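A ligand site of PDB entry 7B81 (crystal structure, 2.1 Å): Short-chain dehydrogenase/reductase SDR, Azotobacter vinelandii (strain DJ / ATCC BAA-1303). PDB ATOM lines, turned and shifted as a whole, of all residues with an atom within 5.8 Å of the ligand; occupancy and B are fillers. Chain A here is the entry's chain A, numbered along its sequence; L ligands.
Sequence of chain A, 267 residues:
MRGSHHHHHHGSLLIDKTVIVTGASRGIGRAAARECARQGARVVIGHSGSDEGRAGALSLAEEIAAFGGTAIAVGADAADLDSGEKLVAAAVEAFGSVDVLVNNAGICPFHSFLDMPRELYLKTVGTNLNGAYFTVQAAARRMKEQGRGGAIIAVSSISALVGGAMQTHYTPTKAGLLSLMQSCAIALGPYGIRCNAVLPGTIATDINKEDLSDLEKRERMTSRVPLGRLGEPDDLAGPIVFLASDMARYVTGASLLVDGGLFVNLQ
CA of Gly 27 touches O7 of the ligand, at 3.6 Å. Ile 28 touches the ligand (CD1 to O9, 3.2 Å). His 47 touches the ligand. N of Ser 48 touches O6 of the ligand (3.9 Å). Ala 76 touches the ligand. CB of Ala 105 touches N5 of the ligand, at 3.6 Å. CG2 of Ile 107 touches N2 of the ligand, at 3.5 Å. Thr 127 touches the ligand (CG2 to N3, 3.3 Å). Val 155 touches the ligand (CG1 to O11, 3.3 Å). Ser 156 touches the ligand (O to C21, 3.3 Å). OG of Ser 157 touches C20 of the ligand (3.2 Å). Pro 200 touches the ligand. O of Gly 201 touches C19 of the ligand, at 3.2 Å. Thr 202 touches the ligand. Asp 206 touches the ligand (N to O2, 3.6 Å). Hydrophobic or aromatic side chains within 4 Å of the ligand: Ile 28, Ala 78, Ala 105, Ile 107, Val 155, Tyr 170, Pro 200, Ile 203 and Ile 207. 28 residues have an atom within 4 Å of the ligand: Gly 23, Ser 25, Arg 26, Gly 27, Ile 28, His 47, Ser 48, Ala 76, Asp 77, Ala 78, Asn 104, Ala 105, Gly 106, Ile 107, Thr 127, Val 155, Ser 156, Ser 157, Tyr 170, Lys 174, Pro 200, Gly 201, Thr 202, Ile 203, Thr 205, Asp 206, Ile 207 and Asn 208. Along chain A the residues within 4 Å of the ligand span positions 23 to 208.
OD2 of Asp 206 is in salt-bridge range of NE of Arg 26, 3.8 Å away. The side-chain carboxylate (OD1) of Asp 77 lies within hydrogen-bond range of the backbone NH (N) of Ala 79. The backbone carbonyl oxygen of Val 155 sits at hydrogen-bond distance from the side-chain amino group of Lys 174, at 3.3 Å. The backbone NH (N) of Ala 76 sits at hydrogen-bond distance from the backbone carbonyl oxygen (O) of His 47. The side-chain amide oxygen (OD1) of Asn 104 sits at hydrogen-bond distance from the backbone NH (N) of Gly 29 (3.4 Å). O of Pro 200 sits at hydrogen-bond distance from N of Ile 158 (3.0 Å). The side-chain hydroxyl (OG) of Ser 157 lies within hydrogen-bond range of the backbone NH (N) of Ser 159 (2.7 Å). The side-chain hydroxyl (OG1) of Thr 22 is in hydrogen-bond range of the backbone NH (N) of Ala 105.
O12 of the ligand lies close to N of Gly 106, 3.5 Å away. N of Arg 26 sits at hydrogen-bond distance from O5 of the ligand (3.3 Å). O of Arg 26 sits at hydrogen-bond distance from O5 of the ligand, at 3.2 Å. NZ of Lys 174 is in hydrogen-bond range of O13 of the ligand. The guanidinium group of Arg 26 is in salt-bridge range of an oxygen (O2) of the ligand (2.8 Å). OG of Ser 25 is in hydrogen-bond range of O6 of the ligand (2.7 Å). N7 of the ligand lies within hydrogen-bond range of O of Ile 203. An oxygen (O1) of the ligand sits close to the backbone NH (N) of Ile 207, 3.4 Å away. The side-chain hydroxyl (OG1) of Thr 205 is in hydrogen-bond range of a nitrogen (N7) of the ligand (3.3 Å). The backbone carbonyl oxygen (O) of Gly 23 sits at hydrogen-bond distance from an oxygen (O5) of the ligand (3.2 Å). ND2 of Asn 208 lies within hydrogen-bond range of O14 of the ligand. A nitrogen (N4) of the ligand is in hydrogen-bond range of the backbone NH (N) of Ala 78, 2.9 Å away. The backbone carbonyl oxygen (O) of Asn 104 sits at hydrogen-bond distance from an oxygen (O12) of the ligand (2.7 Å). The backbone NH of Ile 203 is in hydrogen-bond range of an oxygen (O14) of the ligand, 3.0 Å away. O13 of the ligand is in hydrogen-bond range of OH of Tyr 170, at 2.9 Å. The side-chain carboxylate (OD1) of Asp 77 lies within hydrogen-bond range of a nitrogen (N3) of the ligand (2.9 Å).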
ATOM      1  N   THR A  22      15.618  26.800   4.386  1.00  0.00           N
ATOM      2  CA  THR A  22      16.933  27.405   4.435  1.00  0.00           C
ATOM      3  C   THR A  22      17.488  27.574   3.020  1.00  0.00           C
ATOM      4  O   THR A  22      17.061  26.898   2.078  1.00  0.00           O
ATOM      5  CB  THR A  22      17.889  26.555   5.272  1.00  0.00           C
ATOM      6  OG1 THR A  22      17.901  25.213   4.780  1.00  0.00           O
ATOM      7  CG2 THR A  22      17.474  26.554   6.732  1.00  0.00           C
ATOM      8  N   GLY A  23      18.436  28.489   2.885  1.00  0.00           N
ATOM      9  CA  GLY A  23      19.028  28.760   1.578  1.00  0.00           C
ATOM     10  C   GLY A  23      18.011  29.003   0.492  1.00  0.00           C
ATOM     11  O   GLY A  23      18.149  28.470  -0.627  1.00  0.00           O
ATOM     12  N   ALA A  24      16.978  29.782   0.789  1.00  0.00           N
ATOM     13  CA  ALA A  24      15.940  30.072  -0.186  1.00  0.00           C
ATOM     14  C   ALA A  24      16.173  31.365  -0.947  1.00  0.00           C
ATOM     15  O   ALA A  24      15.327  31.754  -1.760  1.00  0.00           O
ATOM     16  CB  ALA A  24      14.571  30.120   0.507  1.00  0.00           C
ATOM     17  N   SER A  25      17.299  32.042  -0.702  1.00  0.00           N
ATOM     18  CA  SER A  25      17.575  33.281  -1.431  1.00  0.00           C
ATOM     19  C   SER A  25      17.767  33.018  -2.917  1.00  0.00           C
ATOM     20  O   SER A  25      17.333  33.830  -3.748  1.00  0.00           O
ATOM     21  CB  SER A  25      18.807  33.967  -0.830  1.00  0.00           C
ATOM     22  OG  SER A  25      19.831  33.029  -0.544  1.00  0.00           O
ATOM     23  N   ARG A  26      18.397  31.905  -3.269  1.00  0.00           N
ATOM     24  CA  ARG A  26      18.633  31.589  -4.673  1.00  0.00           C
ATOM     25  C   ARG A  26      18.588  30.083  -4.869  1.00  0.00           C
ATOM     26  O   ARG A  26      18.695  29.304  -3.921  1.00  0.00           O
ATOM     27  CB  ARG A  26      19.971  32.155  -5.161  1.00  0.00           C
ATOM     28  CG  ARG A  26      21.211  31.469  -4.576  1.00  0.00           C
ATOM     29  CD  ARG A  26      22.489  32.174  -5.002  1.00  0.00           C
ATOM     30  NE  ARG A  26      23.634  31.282  -5.087  1.00  0.00           N
ATOM     31  CZ  ARG A  26      24.623  31.237  -4.201  1.00  0.00           C
ATOM     32  NH1 ARG A  26      24.622  32.067  -3.158  1.00  0.00           N
ATOM     33  NH2 ARG A  26      25.630  30.384  -4.363  1.00  0.00           N
ATOM     34  N   GLY A  27      18.413  29.688  -6.132  1.00  0.00           N
ATOM     35  CA  GLY A  27      18.578  28.291  -6.497  1.00  0.00           C
ATOM     36  C   GLY A  27      17.378  27.433  -6.144  1.00  0.00           C
ATOM     37  O   GLY A  27      16.217  27.862  -6.225  1.00  0.00           O
ATOM     38  N   ILE A  28      17.664  26.190  -5.766  1.00  0.00           N
ATOM     39  CA  ILE A  28      16.603  25.234  -5.452  1.00  0.00           C
ATOM     40  C   ILE A  28      15.748  25.749  -4.307  1.00  0.00           C
ATOM     41  O   ILE A  28      14.517  25.611  -4.326  1.00  0.00           O
ATOM     42  CB  ILE A  28      17.223  23.852  -5.141  1.00  0.00           C
ATOM     43  CG1 ILE A  28      17.753  23.200  -6.425  1.00  0.00           C
ATOM     44  CG2 ILE A  28      16.225  22.937  -4.453  1.00  0.00           C
ATOM     45  CD1 ILE A  28      18.573  21.949  -6.180  1.00  0.00           C
ATOM     46  N   GLY A  29      16.377  26.351  -3.297  1.00  0.00           N
ATOM     47  CA  GLY A  29      15.622  26.836  -2.153  1.00  0.00           C
ATOM     48  C   GLY A  29      14.591  27.889  -2.520  1.00  0.00           C
ATOM     49  O   GLY A  29      13.482  27.894  -1.997  1.00  0.00           O
ATOM     50  N   GLY A  46      14.715  31.504   5.009  1.00  0.00           N
ATOM     51  CA  GLY A  46      16.019  31.795   5.549  1.00  0.00           C
ATOM     52  C   GLY A  46      17.029  32.046   4.448  1.00  0.00           C
ATOM     53  O   GLY A  46      16.848  31.662   3.300  1.00  0.00           O
ATOM     54  N   HIS A  47      18.121  32.725   4.801  1.00  0.00           N
ATOM     55  CA  HIS A  47      19.147  33.023   3.806  1.00  0.00           C
ATOM     56  C   HIS A  47      20.493  33.187   4.514  1.00  0.00           C
ATOM     57  O   HIS A  47      20.622  32.928   5.709  1.00  0.00           O
ATOM     58  CB  HIS A  47      18.771  34.240   2.961  1.00  0.00           C
ATOM     59  CG  HIS A  47      18.493  35.472   3.765  1.00  0.00           C
ATOM     60  ND1 HIS A  47      19.488  36.229   4.340  1.00  0.00           N
ATOM     61  CD2 HIS A  47      17.334  36.104   4.070  1.00  0.00           C
ATOM     62  CE1 HIS A  47      18.952  37.265   4.974  1.00  0.00           C
ATOM     63  NE2 HIS A  47      17.645  37.207   4.820  1.00  0.00           N
ATOM     64  N   SER A  48      21.495  33.628   3.751  1.00  0.00           N
ATOM     65  CA  SER A  48      22.879  33.688   4.217  1.00  0.00           C
ATOM     66  C   SER A  48      23.091  34.746   5.287  1.00  0.00           C
ATOM     67  O   SER A  48      24.086  34.670   6.013  1.00  0.00           O
ATOM     68  CB  SER A  48      23.806  33.948   3.029  1.00  0.00           C
ATOM     69  OG  SER A  48      25.151  33.626   3.321  1.00  0.00           O
ATOM     70  N   GLY A  53      21.912  37.726  -0.334  1.00  0.00           N
ATOM     71  CA  GLY A  53      20.937  36.755   0.092  1.00  0.00           C
ATOM     72  C   GLY A  53      19.676  37.403   0.636  1.00  0.00           C
ATOM     73  O   GLY A  53      18.567  36.900   0.412  1.00  0.00           O
ATOM     74  N   ALA A  76      20.160  33.714   8.623  1.00  0.00           N
ATOM     75  CA  ALA A  76      20.680  32.739   9.590  1.00  0.00           C
ATOM     76  C   ALA A  76      21.780  31.937   8.923  1.00  0.00           C
ATOM     77  O   ALA A  76      21.513  31.205   7.962  1.00  0.00           O
ATOM     78  CB  ALA A  76      19.567  31.824  10.095  1.00  0.00           C
ATOM     79  N   ASP A  77      23.001  32.075   9.417  1.00  0.00           N
ATOM     80  CA  ASP A  77      24.114  31.289   8.900  1.00  0.00           C
ATOM     81  C   ASP A  77      23.964  29.834   9.328  1.00  0.00           C
ATOM     82  O   ASP A  77      23.927  29.539  10.530  1.00  0.00           O
ATOM     83  CB  ASP A  77      25.444  31.863   9.397  1.00  0.00           C
ATOM     84  CG  ASP A  77      26.619  31.436   8.550  1.00  0.00           C
ATOM     85  OD1 ASP A  77      26.678  30.248   8.160  1.00  0.00           O
ATOM     86  OD2 ASP A  77      27.493  32.287   8.258  1.00  0.00           O
ATOM     87  N   ALA A  78      23.885  28.931   8.343  1.00  0.00           N
ATOM     88  CA  ALA A  78      23.734  27.511   8.652  1.00  0.00           C
ATOM     89  C   ALA A  78      24.947  26.952   9.385  1.00  0.00           C
ATOM     90  O   ALA A  78      24.808  26.028  10.195  1.00  0.00           O
ATOM     91  CB  ALA A  78      23.470  26.723   7.369  1.00  0.00           C
ATOM     92  N   ALA A  79      26.133  27.503   9.118  1.00  0.00           N
ATOM     93  CA  ALA A  79      27.320  27.085   9.872  1.00  0.00           C
ATOM     94  C   ALA A  79      27.178  27.425  11.348  1.00  0.00           C
ATOM     95  O   ALA A  79      27.790  26.758  12.196  1.00  0.00           O
ATOM     96  CB  ALA A  79      28.577  27.718   9.288  1.00  0.00           C
ATOM     97  N   ASN A 104      17.827  23.074   2.982  1.00  0.00           N
ATOM     98  CA  ASN A 104      18.353  23.243   1.639  1.00  0.00           C
ATOM     99  C   ASN A 104      19.712  23.929   1.603  1.00  0.00           C
ATOM    100  O   ASN A 104      20.457  23.729   0.633  1.00  0.00           O
ATOM    101  CB  ASN A 104      17.347  24.045   0.789  1.00  0.00           C
ATOM    102  CG  ASN A 104      17.866  24.364  -0.594  1.00  0.00           C
ATOM    103  OD1 ASN A 104      17.591  23.637  -1.556  1.00  0.00           O
ATOM    104  ND2 ASN A 104      18.585  25.475  -0.714  1.00  0.00           N
ATOM    105  N   ALA A 105      20.063  24.708   2.630  1.00  0.00           N
ATOM    106  CA  ALA A 105      21.310  25.457   2.630  1.00  0.00           C
ATOM    107  C   ALA A 105      22.507  24.528   2.529  1.00  0.00           C
ATOM    108  O   ALA A 105      22.669  23.618   3.354  1.00  0.00           O
ATOM    109  CB  ALA A 105      21.404  26.309   3.893  1.00  0.00           C
ATOM    110  N   GLY A 106      23.343  24.740   1.516  1.00  0.00           N
ATOM    111  CA  GLY A 106      24.520  23.924   1.326  1.00  0.00           C
ATOM    112  C   GLY A 106      25.474  24.585   0.364  1.00  0.00           C
ATOM    113  O   GLY A 106      25.060  25.324  -0.542  1.00  0.00           O
ATOM    114  N   ILE A 107      26.764  24.311   0.553  1.00  0.00           N
ATOM    115  CA  ILE A 107      27.808  24.822  -0.313  1.00  0.00           C
ATOM    116  C   ILE A 107      28.520  23.658  -0.969  1.00  0.00           C
ATOM    117  O   ILE A 107      28.615  22.565  -0.393  1.00  0.00           O
ATOM    118  CB  ILE A 107      28.814  25.709   0.456  1.00  0.00           C
ATOM    119  CG1 ILE A 107      29.358  24.962   1.672  1.00  0.00           C
ATOM    120  CG2 ILE A 107      28.165  27.027   0.863  1.00  0.00           C
ATOM    121  CD1 ILE A 107      30.546  25.638   2.331  1.00  0.00           C
ATOM    122  N   CYS A 108      29.009  23.886  -2.191  1.00  0.00           N
ATOM    123  CA  CYS A 108      29.835  22.909  -2.903  1.00  0.00           C
ATOM    124  C   CYS A 108      31.026  23.640  -3.509  1.00  0.00           C
ATOM    125  O   CYS A 108      31.016  24.021  -4.692  1.00  0.00           O
ATOM    126  CB  CYS A 108      29.029  22.185  -3.979  1.00  0.00           C
ATOM    127  SG  CYS A 108      29.840  20.706  -4.642  1.00  0.00           S
ATOM    128  N   THR A 127      28.403  23.467   7.345  1.00  0.00           N
ATOM    129  CA  THR A 127      27.314  24.172   6.662  1.00  0.00           C
ATOM    130  C   THR A 127      26.264  23.217   6.120  1.00  0.00           C
ATOM    131  O   THR A 127      25.072  23.546   6.121  1.00  0.00           O
ATOM    132  CB  THR A 127      27.874  25.025   5.530  1.00  0.00           C
ATOM    133  OG1 THR A 127      29.034  25.731   5.968  1.00  0.00           O
ATOM    134  CG2 THR A 127      26.831  26.016   5.040  1.00  0.00           C
ATOM    135  N   ASN A 128      26.682  22.055   5.621  1.00  0.00           N
ATOM    136  CA  ASN A 128      25.736  21.156   4.977  1.00  0.00           C
ATOM    137  C   ASN A 128      25.198  20.091   5.915  1.00  0.00           C
ATOM    138  O   ASN A 128      24.057  19.659   5.759  1.00  0.00           O
ATOM    139  CB  ASN A 128      26.403  20.482   3.766  1.00  0.00           C
ATOM    140  CG  ASN A 128      26.912  21.488   2.745  1.00  0.00           C
ATOM    141  OD1 ASN A 128      27.025  22.688   3.033  1.00  0.00           O
ATOM    142  ND2 ASN A 128      27.238  21.005   1.552  1.00  0.00           N
ATOM    143  N   VAL A 155      17.436  18.450   1.269  1.00  0.00           N
ATOM    144  CA  VAL A 155      17.920  18.460  -0.101  1.00  0.00           C
ATOM    145  C   VAL A 155      19.291  17.803  -0.086  1.00  0.00           C
ATOM    146  O   VAL A 155      20.303  18.454   0.173  1.00  0.00           O
ATOM    147  CB  VAL A 155      17.959  19.864  -0.698  1.00  0.00           C
ATOM    148  CG1 VAL A 155      18.542  19.825  -2.116  1.00  0.00           C
ATOM    149  CG2 VAL A 155      16.573  20.481  -0.704  1.00  0.00           C
ATOM    150  N   SER A 156      19.331  16.496  -0.337  1.00  0.00           N
ATOM    151  CA  SER A 156      20.597  15.774  -0.458  1.00  0.00           C
ATOM    152  C   SER A 156      21.075  15.883  -1.906  1.00  0.00           C
ATOM    153  O   SER A 156      21.023  16.960  -2.504  1.00  0.00           O
ATOM    154  CB  SER A 156      20.422  14.321  -0.018  1.00  0.00           C
ATOM    155  OG  SER A 156      21.577  13.546  -0.322  1.00  0.00           O
ATOM    156  N   SER A 157      21.532  14.770  -2.496  1.00  0.00           N
ATOM    157  CA  SER A 157      22.009  14.827  -3.871  1.00  0.00           C
ATOM    158  C   SER A 157      22.090  13.415  -4.436  1.00  0.00           C
ATOM    159  O   SER A 157      22.073  12.429  -3.705  1.00  0.00           O
ATOM    160  CB  SER A 157      23.394  15.476  -3.961  1.00  0.00           C
ATOM    161  OG  SER A 157      23.993  15.206  -5.215  1.00  0.00           O
ATOM    162  N   ILE A 158      22.181  13.354  -5.776  1.00  0.00           N
ATOM    163  CA  ILE A 158      22.558  12.108  -6.424  1.00  0.00           C
ATOM    164  C   ILE A 158      23.943  11.679  -5.955  1.00  0.00           C
ATOM    165  O   ILE A 158      24.238  10.489  -5.854  1.00  0.00           O
ATOM    166  CB  ILE A 158      22.481  12.250  -7.959  1.00  0.00           C
ATOM    167  CG1 ILE A 158      22.921  10.955  -8.648  1.00  0.00           C
ATOM    168  CG2 ILE A 158      23.313  13.443  -8.422  1.00  0.00           C
ATOM    169  CD1 ILE A 158      22.895  11.050 -10.168  1.00  0.00           C
ATOM    170  N   SER A 159      24.792  12.660  -5.615  1.00  0.00           N
ATOM    171  CA  SER A 159      26.112  12.401  -5.034  1.00  0.00           C
ATOM    172  C   SER A 159      26.045  11.695  -3.683  1.00  0.00           C
ATOM    173  O   SER A 159      27.100  11.362  -3.128  1.00  0.00           O
ATOM    174  CB  SER A 159      26.879  13.711  -4.881  1.00  0.00           C
ATOM    175  OG  SER A 159      27.103  14.335  -6.141  1.00  0.00           O
ATOM    176  N   TYR A 170      32.364  17.133  -0.122  1.00  0.00           N
ATOM    177  CA  TYR A 170      30.959  17.486  -0.331  1.00  0.00           C
ATOM    178  C   TYR A 170      30.028  16.281  -0.259  1.00  0.00           C
ATOM    179  O   TYR A 170      29.017  16.337   0.440  1.00  0.00           O
ATOM    180  CB  TYR A 170      30.826  18.192  -1.687  1.00  0.00           C
ATOM    181  CG  TYR A 170      29.409  18.411  -2.154  1.00  0.00           C
ATOM    182  CD1 TYR A 170      28.606  19.392  -1.588  1.00  0.00           C
ATOM    183  CD2 TYR A 170      28.882  17.665  -3.208  1.00  0.00           C
ATOM    184  CE1 TYR A 170      27.311  19.605  -2.032  1.00  0.00           C
ATOM    185  CE2 TYR A 170      27.592  17.865  -3.655  1.00  0.00           C
ATOM    186  CZ  TYR A 170      26.813  18.835  -3.070  1.00  0.00           C
ATOM    187  OH  TYR A 170      25.527  19.039  -3.526  1.00  0.00           O
ATOM    188  N   LYS A 174      26.232  15.175   1.938  1.00  0.00           N
ATOM    189  CA  LYS A 174      24.946  14.835   1.346  1.00  0.00           C
ATOM    190  C   LYS A 174      24.539  13.402   1.700  1.00  0.00           C
ATOM    191  O   LYS A 174      23.368  13.136   1.982  1.00  0.00           O
ATOM    192  CB  LYS A 174      24.975  15.023  -0.173  1.00  0.00           C
ATOM    193  CG  LYS A 174      25.782  16.231  -0.642  1.00  0.00           C
ATOM    194  CD  LYS A 174      25.334  17.527   0.033  1.00  0.00           C
ATOM    195  CE  LYS A 174      23.907  17.889  -0.319  1.00  0.00           C
ATOM    196  NZ  LYS A 174      23.491  19.168   0.325  1.00  0.00           N
ATOM    197  N   PRO A 200      18.564  15.506  -5.902  1.00  0.00           N
ATOM    198  CA  PRO A 200      18.593  16.140  -7.222  1.00  0.00           C
ATOM    199  C   PRO A 200      19.844  15.781  -8.009  1.00  0.00           C
ATOM    200  O   PRO A 200      20.917  15.557  -7.452  1.00  0.00           O
ATOM    201  CB  PRO A 200      18.559  17.641  -6.897  1.00  0.00           C
ATOM    202  CG  PRO A 200      19.187  17.734  -5.550  1.00  0.00           C
ATOM    203  CD  PRO A 200      18.801  16.474  -4.814  1.00  0.00           C
ATOM    204  N   GLY A 201      19.668  15.701  -9.324  1.00  0.00           N
ATOM    205  CA  GLY A 201      20.783  15.400 -10.201  1.00  0.00           C
ATOM    206  C   GLY A 201      21.612  16.634 -10.485  1.00  0.00           C
ATOM    207  O   GLY A 201      21.860  17.449  -9.591  1.00  0.00           O
ATOM    208  N   THR A 202      22.041  16.792 -11.737  1.00  0.00           N
ATOM    209  CA  THR A 202      22.772  17.976 -12.146  1.00  0.00           C
ATOM    210  C   THR A 202      21.759  19.086 -12.439  1.00  0.00           C
ATOM    211  O   THR A 202      21.043  19.030 -13.443  1.00  0.00           O
ATOM    212  CB  THR A 202      23.641  17.676 -13.360  1.00  0.00           C
ATOM    213  OG1 THR A 202      24.571  16.639 -13.025  1.00  0.00           O
ATOM    214  CG2 THR A 202      24.415  18.923 -13.790  1.00  0.00           C
ATOM    215  N   ILE A 203      21.677  20.063 -11.549  1.00  0.00           N
ATOM    216  CA  ILE A 203      20.749  21.180 -11.671  1.00  0.00           C
ATOM    217  C   ILE A 203      21.551  22.428 -12.011  1.00  0.00           C
ATOM    218  O   ILE A 203      22.528  22.742 -11.322  1.00  0.00           O
ATOM    219  CB  ILE A 203      19.924  21.382 -10.384  1.00  0.00           C
ATOM    220  CG1 ILE A 203      19.474  20.033  -9.812  1.00  0.00           C
ATOM    221  CG2 ILE A 203      18.734  22.286 -10.649  1.00  0.00           C
ATOM    222  CD1 ILE A 203      18.532  19.262 -10.724  1.00  0.00           C
ATOM    223  N   ALA A 204      21.144  23.120 -13.073  1.00  0.00           N
ATOM    224  CA  ALA A 204      21.848  24.318 -13.538  1.00  0.00           C
ATOM    225  C   ALA A 204      21.516  25.470 -12.593  1.00  0.00           C
ATOM    226  O   ALA A 204      20.521  26.182 -12.767  1.00  0.00           O
ATOM    227  CB  ALA A 204      21.469  24.643 -14.979  1.00  0.00           C
ATOM    228  N   THR A 205      22.355  25.652 -11.585  1.00  0.00           N
ATOM    229  CA  THR A 205      22.239  26.763 -10.659  1.00  0.00           C
ATOM    230  C   THR A 205      23.576  27.507 -10.652  1.00  0.00           C
ATOM    231  O   THR A 205      24.370  27.420 -11.590  1.00  0.00           O
ATOM    232  CB  THR A 205      21.835  26.287  -9.257  1.00  0.00           C
ATOM    233  OG1 THR A 205      22.960  25.691  -8.600  1.00  0.00           O
ATOM    234  CG2 THR A 205      20.693  25.291  -9.325  1.00  0.00           C
ATOM    235  N   ASP A 206      23.821  28.245  -9.577  1.00  0.00           N
ATOM    236  CA  ASP A 206      25.105  28.911  -9.378  1.00  0.00           C
ATOM    237  C   ASP A 206      26.049  28.094  -8.506  1.00  0.00           C
ATOM    238  O   ASP A 206      27.188  28.525  -8.291  1.00  0.00           O
ATOM    239  CB  ASP A 206      24.896  30.305  -8.765  1.00  0.00           C
ATOM    240  CG  ASP A 206      23.819  31.096  -9.484  1.00  0.00           C
ATOM    241  OD1 ASP A 206      23.607  30.859 -10.688  1.00  0.00           O
ATOM    242  OD2 ASP A 206      23.195  31.969  -8.843  1.00  0.00           O
ATOM    243  N   ILE A 207      25.620  26.928  -8.017  1.00  0.00           N
ATOM    244  CA  ILE A 207      26.546  26.028  -7.345  1.00  0.00           C
ATOM    245  C   ILE A 207      27.556  25.469  -8.344  1.00  0.00           C
ATOM    246  O   ILE A 207      28.651  25.038  -7.966  1.00  0.00           O
ATOM    247  CB  ILE A 207      25.773  24.887  -6.627  1.00  0.00           C
ATOM    248  CG1 ILE A 207      26.541  24.400  -5.399  1.00  0.00           C
ATOM    249  CG2 ILE A 207      25.467  23.735  -7.584  1.00  0.00           C
ATOM    250  CD1 ILE A 207      25.815  23.321  -4.614  1.00  0.00           C
ATOM    251  N   ASN A 208      27.193  25.481  -9.636  1.00  0.00           N
ATOM    252  CA  ASN A 208      28.019  24.894 -10.683  1.00  0.00           C
ATOM    253  C   ASN A 208      28.026  25.774 -11.929  1.00  0.00           C
ATOM    254  O   ASN A 208      28.183  25.272 -13.048  1.00  0.00           O
ATOM    255  CB  ASN A 208      27.521  23.487 -11.029  1.00  0.00           C
ATOM    256  CG  ASN A 208      26.001  23.414 -11.178  1.00  0.00           C
ATOM    257  OD1 ASN A 208      25.321  24.439 -11.216  1.00  0.00           O
ATOM    258  ND2 ASN A 208      25.479  22.198 -11.268  1.00  0.00           N
HETATM  259  P1  LIG L   1      22.823  27.700  -5.054  1.00  0.00           P
HETATM  260  O1  LIG L   1      24.147  27.015  -4.955  1.00  0.00           O
HETATM  261  O2  LIG L   1      22.883  28.775  -6.113  1.00  0.00           O
HETATM  262  O3  LIG L   1      22.463  28.370  -3.575  1.00  0.00           O
HETATM  263  C1  LIG L   1      22.580  27.557  -2.441  1.00  0.00           C
HETATM  264  C2  LIG L   1      21.773  28.205  -1.255  1.00  0.00           C
HETATM  265  O4  LIG L   1      22.308  27.863  -0.137  1.00  0.00           O
HETATM  266  C3  LIG L   1      21.883  29.732  -1.359  1.00  0.00           C
HETATM  267  O5  LIG L   1      20.658  30.274  -1.540  1.00  0.00           O
HETATM  268  C4  LIG L   1      22.509  30.208  -0.032  1.00  0.00           C
HETATM  269  O6  LIG L   1      21.737  31.400   0.533  1.00  0.00           O
HETATM  270  C5  LIG L   1      22.411  29.215   0.777  1.00  0.00           C
HETATM  271  N1  LIG L   1      23.567  29.140   1.637  1.00  0.00           N
HETATM  272  C6  LIG L   1      24.823  28.842   1.266  1.00  0.00           C
HETATM  273  N2  LIG L   1      25.585  28.872   2.367  1.00  0.00           N
HETATM  274  C7  LIG L   1      24.813  29.191   3.407  1.00  0.00           C
HETATM  275  C8  LIG L   1      25.085  29.358   4.742  1.00  0.00           C
HETATM  276  N3  LIG L   1      26.340  29.243   5.472  1.00  0.00           N
HETATM  277  N4  LIG L   1      24.109  29.683   5.592  1.00  0.00           N
HETATM  278  C9  LIG L   1      22.846  29.847   5.141  1.00  0.00           C
HETATM  279  N5  LIG L   1      22.560  29.684   3.826  1.00  0.00           N
HETATM  280  C10 LIG L   1      23.559  29.350   2.958  1.00  0.00           C
HETATM  281  O7  LIG L   1      21.634  26.616  -5.425  1.00  0.00           O
HETATM  282  P2  LIG L   1      21.670  24.998  -4.994  1.00  0.00           P
HETATM  283  O8  LIG L   1      23.050  24.430  -5.214  1.00  0.00           O
HETATM  284  O9  LIG L   1      20.713  24.252  -5.877  1.00  0.00           O
HETATM  285  O10 LIG L   1      21.296  24.787  -3.433  1.00  0.00           O
HETATM  286  C11 LIG L   1      20.247  23.894  -3.105  1.00  0.00           C
HETATM  287  C12 LIG L   1      20.792  22.532  -2.614  1.00  0.00           C
HETATM  288  O11 LIG L   1      20.805  21.678  -3.613  1.00  0.00           O
HETATM  289  C13 LIG L   1      22.250  22.616  -2.098  1.00  0.00           C
HETATM  290  O12 LIG L   1      22.282  22.361  -0.778  1.00  0.00           O
HETATM  291  C14 LIG L   1      23.030  21.502  -2.865  1.00  0.00           C
HETATM  292  O13 LIG L   1      23.902  20.734  -1.908  1.00  0.00           O
HETATM  293  C15 LIG L   1      22.086  20.720  -3.365  1.00  0.00           C
HETATM  294  N6  LIG L   1      22.438  20.125  -4.601  1.00  0.00           N
HETATM  295  C16 LIG L   1      22.514  20.891  -5.769  1.00  0.00           C
HETATM  296  C17 LIG L   1      22.839  20.258  -6.989  1.00  0.00           C
HETATM  297  C18 LIG L   1      22.952  21.042  -8.277  1.00  0.00           C
HETATM  298  O14 LIG L   1      23.492  20.553  -9.214  1.00  0.00           O
HETATM  299  N7  LIG L   1      22.363  22.415  -8.378  1.00  0.00           N
HETATM  300  C19 LIG L   1      23.072  18.913  -7.035  1.00  0.00           C
HETATM  301  C20 LIG L   1      22.984  18.161  -5.878  1.00  0.00           C
HETATM  302  C21 LIG L   1      22.654  18.790  -4.650  1.00  0.00           C
